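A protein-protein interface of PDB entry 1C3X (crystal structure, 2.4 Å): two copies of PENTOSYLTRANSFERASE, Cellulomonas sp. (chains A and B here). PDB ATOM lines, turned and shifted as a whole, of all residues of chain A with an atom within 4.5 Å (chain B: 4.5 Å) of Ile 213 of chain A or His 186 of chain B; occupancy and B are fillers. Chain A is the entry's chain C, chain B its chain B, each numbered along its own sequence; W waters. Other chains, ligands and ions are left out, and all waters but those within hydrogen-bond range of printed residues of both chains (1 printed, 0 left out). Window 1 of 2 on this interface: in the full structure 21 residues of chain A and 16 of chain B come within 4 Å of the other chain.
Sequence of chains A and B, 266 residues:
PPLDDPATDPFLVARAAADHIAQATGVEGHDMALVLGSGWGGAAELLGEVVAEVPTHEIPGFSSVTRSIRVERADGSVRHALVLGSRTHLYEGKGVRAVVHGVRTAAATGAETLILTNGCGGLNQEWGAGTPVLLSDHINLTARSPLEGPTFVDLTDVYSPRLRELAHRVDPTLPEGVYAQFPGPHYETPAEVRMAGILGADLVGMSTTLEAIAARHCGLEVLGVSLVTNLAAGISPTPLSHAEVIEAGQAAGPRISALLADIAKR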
ATOM      1  N   HIS A 138       3.747   6.039 -10.348  1.00  0.00           N
ATOM      2  CA  HIS A 138       4.855   5.650 -11.218  1.00  0.00           C
ATOM      3  C   HIS A 138       5.688   6.844 -11.714  1.00  0.00           C
ATOM      4  O   HIS A 138       5.317   8.008 -11.551  1.00  0.00           O
ATOM      5  CB  HIS A 138       4.332   4.889 -12.412  1.00  0.00           C
ATOM      6  CG  HIS A 138       3.553   5.742 -13.356  1.00  0.00           C
ATOM      7  ND1 HIS A 138       2.453   5.276 -14.042  1.00  0.00           N
ATOM      8  CD2 HIS A 138       3.733   7.024 -13.760  1.00  0.00           C
ATOM      9  CE1 HIS A 138       1.986   6.236 -14.830  1.00  0.00           C
ATOM     10  NE2 HIS A 138       2.746   7.308 -14.676  1.00  0.00           N
ATOM     11  N   ASN A 140       7.567   7.633 -15.215  1.00  0.00           N
ATOM     12  CA  ASN A 140       7.785   7.220 -16.587  1.00  0.00           C
ATOM     13  C   ASN A 140       9.054   7.882 -17.148  1.00  0.00           C
ATOM     14  O   ASN A 140       9.084   9.087 -17.516  1.00  0.00           O
ATOM     15  CB  ASN A 140       6.545   7.569 -17.387  1.00  0.00           C
ATOM     16  CG  ASN A 140       6.833   7.737 -18.828  1.00  0.00           C
ATOM     17  OD1 ASN A 140       7.726   7.053 -19.371  1.00  0.00           O
ATOM     18  ND2 ASN A 140       6.062   8.625 -19.498  1.00  0.00           N
ATOM     19  N   ARG A 144       8.622   9.262 -23.506  1.00  0.00           N
ATOM     20  CA  ARG A 144       7.550   9.097 -24.500  1.00  0.00           C
ATOM     21  C   ARG A 144       6.166   9.235 -23.843  1.00  0.00           C
ATOM     22  O   ARG A 144       6.040   9.127 -22.617  1.00  0.00           O
ATOM     23  CB  ARG A 144       7.694   7.731 -25.154  1.00  0.00           C
ATOM     24  CG  ARG A 144       8.938   7.643 -26.003  1.00  0.00           C
ATOM     25  CD  ARG A 144       8.775   8.504 -27.272  1.00  0.00           C
ATOM     26  NE  ARG A 144       7.943   7.861 -28.306  1.00  0.00           N
ATOM     27  CZ  ARG A 144       8.252   6.701 -28.898  1.00  0.00           C
ATOM     28  NH1 ARG A 144       9.366   6.050 -28.569  1.00  0.00           N
ATOM     29  NH2 ARG A 144       7.454   6.187 -29.826  1.00  0.00           N
ATOM     30  N   SER A 145       5.147   9.507 -24.652  1.00  0.00           N
ATOM     31  CA  SER A 145       3.781   9.568 -24.126  1.00  0.00           C
ATOM     32  C   SER A 145       2.827   8.888 -25.082  1.00  0.00           C
ATOM     33  O   SER A 145       3.017   8.913 -26.312  1.00  0.00           O
ATOM     34  CB  SER A 145       3.289  10.998 -23.929  1.00  0.00           C
ATOM     35  OG  SER A 145       2.018  10.978 -23.283  1.00  0.00           O
ATOM     36  N   PRO A 146       1.815   8.205 -24.536  1.00  0.00           N
ATOM     37  CA  PRO A 146       0.864   7.557 -25.438  1.00  0.00           C
ATOM     38  C   PRO A 146      -0.139   8.580 -25.996  1.00  0.00           C
ATOM     39  O   PRO A 146      -0.841   8.298 -26.967  1.00  0.00           O
ATOM     40  CB  PRO A 146       0.204   6.512 -24.528  1.00  0.00           C
ATOM     41  CG  PRO A 146       0.160   7.245 -23.198  1.00  0.00           C
ATOM     42  CD  PRO A 146       1.551   7.846 -23.121  1.00  0.00           C
ATOM     43  N   LEU A 147      -0.193   9.774 -25.415  1.00  0.00           N
ATOM     44  CA  LEU A 147      -1.168  10.772 -25.881  1.00  0.00           C
ATOM     45  C   LEU A 147      -0.656  11.647 -27.051  1.00  0.00           C
ATOM     46  O   LEU A 147       0.481  12.124 -27.036  1.00  0.00           O
ATOM     47  CB  LEU A 147      -1.607  11.647 -24.706  1.00  0.00           C
ATOM     48  CG  LEU A 147      -2.052  10.938 -23.406  1.00  0.00           C
ATOM     49  CD1 LEU A 147      -2.616  11.996 -22.444  1.00  0.00           C
ATOM     50  CD2 LEU A 147      -3.139   9.878 -23.684  1.00  0.00           C
ATOM     51  N   VAL A 153      -4.490  15.423 -19.728  1.00  0.00           N
ATOM     52  CA  VAL A 153      -5.157  14.538 -18.722  1.00  0.00           C
ATOM     53  C   VAL A 153      -4.496  14.519 -17.344  1.00  0.00           C
ATOM     54  O   VAL A 153      -3.259  14.404 -17.240  1.00  0.00           O
ATOM     55  CB  VAL A 153      -5.202  13.042 -19.145  1.00  0.00           C
ATOM     56  CG1 VAL A 153      -6.163  12.838 -20.280  1.00  0.00           C
ATOM     57  CG2 VAL A 153      -3.830  12.573 -19.531  1.00  0.00           C
ATOM     58  N   LEU A 155      -3.187  13.065 -13.944  1.00  0.00           N
ATOM     59  CA  LEU A 155      -2.661  11.785 -13.472  1.00  0.00           C
ATOM     60  C   LEU A 155      -2.339  11.819 -11.993  1.00  0.00           C
ATOM     61  O   LEU A 155      -1.283  11.327 -11.543  1.00  0.00           O
ATOM     62  CB  LEU A 155      -1.417  11.466 -14.293  1.00  0.00           C
ATOM     63  CG  LEU A 155      -1.766  11.642 -15.778  1.00  0.00           C
ATOM     64  CD1 LEU A 155      -0.533  11.310 -16.652  1.00  0.00           C
ATOM     65  CD2 LEU A 155      -2.969  10.696 -16.112  1.00  0.00           C
ATOM     66  N   THR A 209       3.536   1.997 -17.349  1.00  0.00           N
ATOM     67  CA  THR A 209       3.140   3.413 -17.218  1.00  0.00           C
ATOM     68  C   THR A 209       2.487   4.058 -18.469  1.00  0.00           C
ATOM     69  O   THR A 209       1.579   4.908 -18.341  1.00  0.00           O
ATOM     70  CB  THR A 209       4.370   4.257 -16.730  1.00  0.00           C
ATOM     71  OG1 THR A 209       5.159   4.699 -17.851  1.00  0.00           O
ATOM     72  CG2 THR A 209       5.293   3.371 -15.860  1.00  0.00           C
ATOM     73  N   LEU A 210       2.938   3.696 -19.671  1.00  0.00           N
ATOM     74  CA  LEU A 210       2.340   4.264 -20.859  1.00  0.00           C
ATOM     75  C   LEU A 210       0.955   3.674 -20.941  1.00  0.00           C
ATOM     76  O   LEU A 210      -0.003   4.392 -21.244  1.00  0.00           O
ATOM     77  CB  LEU A 210       3.116   3.881 -22.114  1.00  0.00           C
ATOM     78  CG  LEU A 210       4.554   4.381 -22.137  1.00  0.00           C
ATOM     79  CD1 LEU A 210       5.158   4.150 -23.518  1.00  0.00           C
ATOM     80  CD2 LEU A 210       4.555   5.870 -21.781  1.00  0.00           C
ATOM     81  N   GLU A 211       0.820   2.367 -20.694  1.00  0.00           N
ATOM     82  CA  GLU A 211      -0.512   1.791 -20.721  1.00  0.00           C
ATOM     83  C   GLU A 211      -1.424   2.548 -19.673  1.00  0.00           C
ATOM     84  O   GLU A 211      -2.536   3.033 -20.016  1.00  0.00           O
ATOM     85  CB  GLU A 211      -0.469   0.283 -20.410  1.00  0.00           C
ATOM     86  CG  GLU A 211       0.304  -0.628 -21.425  1.00  0.00           C
ATOM     87  CD  GLU A 211       1.710  -1.063 -20.962  1.00  0.00           C
ATOM     88  OE1 GLU A 211       2.572  -0.169 -20.794  1.00  0.00           O
ATOM     89  OE2 GLU A 211       1.951  -2.295 -20.764  1.00  0.00           O
ATOM     90  N   ALA A 212      -0.936   2.702 -18.443  1.00  0.00           N
ATOM     91  CA  ALA A 212      -1.698   3.343 -17.367  1.00  0.00           C
ATOM     92  C   ALA A 212      -2.146   4.732 -17.700  1.00  0.00           C
ATOM     93  O   ALA A 212      -3.294   5.135 -17.400  1.00  0.00           O
ATOM     94  CB  ALA A 212      -0.891   3.358 -16.046  1.00  0.00           C
ATOM     95  N   ILE A 213      -1.252   5.491 -18.311  1.00  0.00           N
ATOM     96  CA  ILE A 213      -1.609   6.840 -18.697  1.00  0.00           C
ATOM     97  C   ILE A 213      -2.681   6.699 -19.751  1.00  0.00           C
ATOM     98  O   ILE A 213      -3.645   7.447 -19.768  1.00  0.00           O
ATOM     99  CB  ILE A 213      -0.405   7.585 -19.317  1.00  0.00           C
ATOM    100  CG1 ILE A 213       0.636   7.909 -18.221  1.00  0.00           C
ATOM    101  CG2 ILE A 213      -0.877   8.844 -20.017  1.00  0.00           C
ATOM    102  CD1 ILE A 213       1.988   8.483 -18.781  1.00  0.00           C
ATOM    103  N   ALA A 214      -2.514   5.730 -20.642  1.00  0.00           N
ATOM    104  CA  ALA A 214      -3.486   5.536 -21.713  1.00  0.00           C
ATOM    105  C   ALA A 214      -4.855   5.174 -21.115  1.00  0.00           C
ATOM    106  O   ALA A 214      -5.882   5.772 -21.477  1.00  0.00           O
ATOM    107  CB  ALA A 214      -3.001   4.437 -22.628  1.00  0.00           C
ATOM    108  N   ALA A 215      -4.877   4.211 -20.188  1.00  0.00           N
ATOM    109  CA  ALA A 215      -6.125   3.808 -19.532  1.00  0.00           C
ATOM    110  C   ALA A 215      -6.770   5.041 -18.898  1.00  0.00           C
ATOM    111  O   ALA A 215      -7.937   5.364 -19.192  1.00  0.00           O
ATOM    112  CB  ALA A 215      -5.866   2.741 -18.428  1.00  0.00           C
ATOM    113  N   ARG A 216      -6.012   5.752 -18.056  1.00  0.00           N
ATOM    114  CA  ARG A 216      -6.560   6.905 -17.377  1.00  0.00           C
ATOM    115  C   ARG A 216      -7.183   7.890 -18.342  1.00  0.00           C
ATOM    116  O   ARG A 216      -8.248   8.476 -18.061  1.00  0.00           O
ATOM    117  CB  ARG A 216      -5.496   7.509 -16.497  1.00  0.00           C
ATOM    118  CG  ARG A 216      -5.189   6.627 -15.277  1.00  0.00           C
ATOM    119  CD  ARG A 216      -6.042   7.062 -14.106  1.00  0.00           C
ATOM    120  NE  ARG A 216      -7.469   6.883 -14.393  1.00  0.00           N
ATOM    121  CZ  ARG A 216      -8.463   7.679 -13.976  1.00  0.00           C
ATOM    122  NH1 ARG A 216      -8.249   8.751 -13.205  1.00  0.00           N
ATOM    123  NH2 ARG A 216      -9.707   7.357 -14.280  1.00  0.00           N
ATOM    124  N   HIS A 217      -6.569   8.037 -19.511  1.00  0.00           N
ATOM    125  CA  HIS A 217      -7.128   8.926 -20.532  1.00  0.00           C
ATOM    126  C   HIS A 217      -8.497   8.394 -21.010  1.00  0.00           C
ATOM    127  O   HIS A 217      -9.414   9.165 -21.334  1.00  0.00           O
ATOM    128  CB  HIS A 217      -6.159   9.022 -21.710  1.00  0.00           C
ATOM    129  CG  HIS A 217      -6.674   9.849 -22.849  1.00  0.00           C
ATOM    130  ND1 HIS A 217      -6.868   9.333 -24.114  1.00  0.00           N
ATOM    131  CD2 HIS A 217      -6.974  11.177 -22.926  1.00  0.00           C
ATOM    132  CE1 HIS A 217      -7.262  10.309 -24.928  1.00  0.00           C
ATOM    133  NE2 HIS A 217      -7.335  11.436 -24.234  1.00  0.00           N
ATOM    134  N   GLY B 184       5.505  15.571 -22.360  1.00  0.00           N
ATOM    135  CA  GLY B 184       4.058  15.778 -22.408  1.00  0.00           C
ATOM    136  C   GLY B 184       3.455  14.839 -23.478  1.00  0.00           C
ATOM    137  O   GLY B 184       4.163  13.960 -23.995  1.00  0.00           O
ATOM    138  N   PRO B 185       2.164  14.994 -23.871  1.00  0.00           N
ATOM    139  CA  PRO B 185       1.191  15.970 -23.401  1.00  0.00           C
ATOM    140  C   PRO B 185       0.532  15.625 -22.101  1.00  0.00           C
ATOM    141  O   PRO B 185      -0.205  16.438 -21.550  1.00  0.00           O
ATOM    142  CB  PRO B 185       0.211  16.025 -24.561  1.00  0.00           C
ATOM    143  CG  PRO B 185       0.162  14.585 -24.950  1.00  0.00           C
ATOM    144  CD  PRO B 185       1.614  14.258 -25.032  1.00  0.00           C
ATOM    145  N   HIS B 186       0.765  14.439 -21.581  1.00  0.00           N
ATOM    146  CA  HIS B 186       0.139  14.108 -20.317  1.00  0.00           C
ATOM    147  C   HIS B 186       0.829  14.895 -19.222  1.00  0.00           C
ATOM    148  O   HIS B 186       1.940  15.421 -19.437  1.00  0.00           O
ATOM    149  CB  HIS B 186       0.284  12.640 -20.020  1.00  0.00           C
ATOM    150  CG  HIS B 186       1.699  12.195 -19.845  1.00  0.00           C
ATOM    151  ND1 HIS B 186       2.417  11.589 -20.859  1.00  0.00           N
ATOM    152  CD2 HIS B 186       2.489  12.155 -18.740  1.00  0.00           C
ATOM    153  CE1 HIS B 186       3.584  11.185 -20.377  1.00  0.00           C
ATOM    154  NE2 HIS B 186       3.651  11.516 -19.097  1.00  0.00           N
ATOM    155  N   TYR B 187       0.191  14.967 -18.049  1.00  0.00           N
ATOM    156  CA  TYR B 187       0.727  15.663 -16.880  1.00  0.00           C
ATOM    157  C   TYR B 187       1.472  14.727 -15.960  1.00  0.00           C
ATOM    158  O   TYR B 187       1.372  13.518 -16.100  1.00  0.00           O
ATOM    159  CB  TYR B 187      -0.381  16.358 -16.088  1.00  0.00           C
ATOM    160  CG  TYR B 187      -0.960  17.522 -16.838  1.00  0.00           C
ATOM    161  CD1 TYR B 187      -0.136  18.322 -17.639  1.00  0.00           C
ATOM    162  CD2 TYR B 187      -2.308  17.857 -16.723  1.00  0.00           C
ATOM    163  CE1 TYR B 187      -0.637  19.437 -18.306  1.00  0.00           C
ATOM    164  CE2 TYR B 187      -2.832  18.984 -17.389  1.00  0.00           C
ATOM    165  CZ  TYR B 187      -1.981  19.773 -18.180  1.00  0.00           C
ATOM    166  OH  TYR B 187      -2.457  20.909 -18.823  1.00  0.00           O
ATOM    167  N   GLU B 188       2.198  15.284 -15.001  1.00  0.00           N
ATOM    168  CA  GLU B 188       3.025  14.500 -14.099  1.00  0.00           C
ATOM    169  C   GLU B 188       2.325  13.902 -12.907  1.00  0.00           C
ATOM    170  O   GLU B 188       1.434  14.508 -12.309  1.00  0.00           O
ATOM    171  CB  GLU B 188       4.180  15.349 -13.558  1.00  0.00           C
ATOM    172  CG  GLU B 188       5.104  15.997 -14.587  1.00  0.00           C
ATOM    173  CD  GLU B 188       4.402  17.010 -15.483  1.00  0.00           C
ATOM    174  OE1 GLU B 188       3.656  17.876 -14.951  1.00  0.00           O
ATOM    175  OE2 GLU B 188       4.611  16.946 -16.731  1.00  0.00           O
ATOM    176  N   MET B 206       5.564  21.753 -20.651  1.00  0.00           N
ATOM    177  CA  MET B 206       5.931  20.930 -21.821  1.00  0.00           C
ATOM    178  C   MET B 206       6.411  21.703 -23.037  1.00  0.00           C
ATOM    179  O   MET B 206       6.201  21.294 -24.184  1.00  0.00           O
ATOM    180  CB  MET B 206       4.775  19.973 -22.189  1.00  0.00           C
ATOM    181  CG  MET B 206       3.397  20.582 -22.253  1.00  0.00           C
ATOM    182  SD  MET B 206       2.037  19.342 -22.061  1.00  0.00           S
ATOM    183  CE  MET B 206       2.352  18.638 -20.402  1.00  0.00           C
HETATM  184  O   HOH W   1       3.271   9.787 -16.300  1.00  0.00           O
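A ring nitrogen (ND1) of His 186 of chain B sits at hydrogen-bond distance from the side-chain hydroxyl of Ser 145 of chain A (2.5 Å).
N of Leu 147 of chain A sits close to OG of Ser 145 of chain A (3.3 Å).
The side-chain amide nitrogen (ND2) of Asn 140 of chain A is in hydrogen-bond range of the backbone carbonyl oxygen (O) of Arg 144 of chain A, 3.2 Å away.
CE1 of His 186 of chain B touches ND2 of Asn 140 of chain A, 3.7 Å away.
Arg 144 of chain A touches His 186 of chain B (O to CE1, 3.9 Å).
Ser 145 of chain A touches Gly 184 of chain B.
Ser 145 of chain A touches Pro 185 of chain B.
Pro 185 of chain B touches Leu 147 of chain A.
CB of His 186 of chain B touches CD1 of Leu 147 of chain A, at 3.8 Å.
O of Val 153 of chain A touches N of Tyr 187 of chain B, at 3.6 Å.
His 186 of chain B touches Leu 155 of chain A.
CD1 of Leu 155 of chain A touches O of Tyr 187 of chain B, at 3.0 Å.
NE2 of His 186 of chain B touches CD1 of Ile 213 of chain A (3.5 Å).
Printed residues of chain B within 4 Å of Val 153 of chain A: Tyr 187 (3.6 Å).
Of the printed residues of chain B, Leu 155 of chain A touches His 186 (3.7 Å) and Tyr 187 (3.0 Å).
Ala 215 of chain A touches none of the printed residues of chain B.
Printed residues of chain A within 4 Å of Gly 184 of chain B: Ser 145.
His 186 of chain B touches just these residues of chain A: Asn 140, Arg 144, Ser 145, Leu 147, Leu 155 and Ile 213.
The nearest printed residue of chain B that does not touch Ile 213 of chain A is Tyr 187 of chain B (5.7 Å).
The nearest residue of chain A that does not touch His 186 of chain B is Val 153 of chain A (4.1 Å).
Along chain B the printed residues that touch a printed residue of chain A span positions 184 to 187.
Hydrophobic or aromatic side chains of chain A within 4 Å of the printed part of chain B: Leu 147, Leu 155 and Ile 213.
No position is printed for both chains.
Of the 11 pairs that touch across the chains among the printed residues, none has its exchanged pair printed and touching as well.
Water W1 lies within hydrogen-bond range of a ring nitrogen (NE2) of His 138 of chain A and a ring nitrogen (NE2) of His 186 of chain B.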
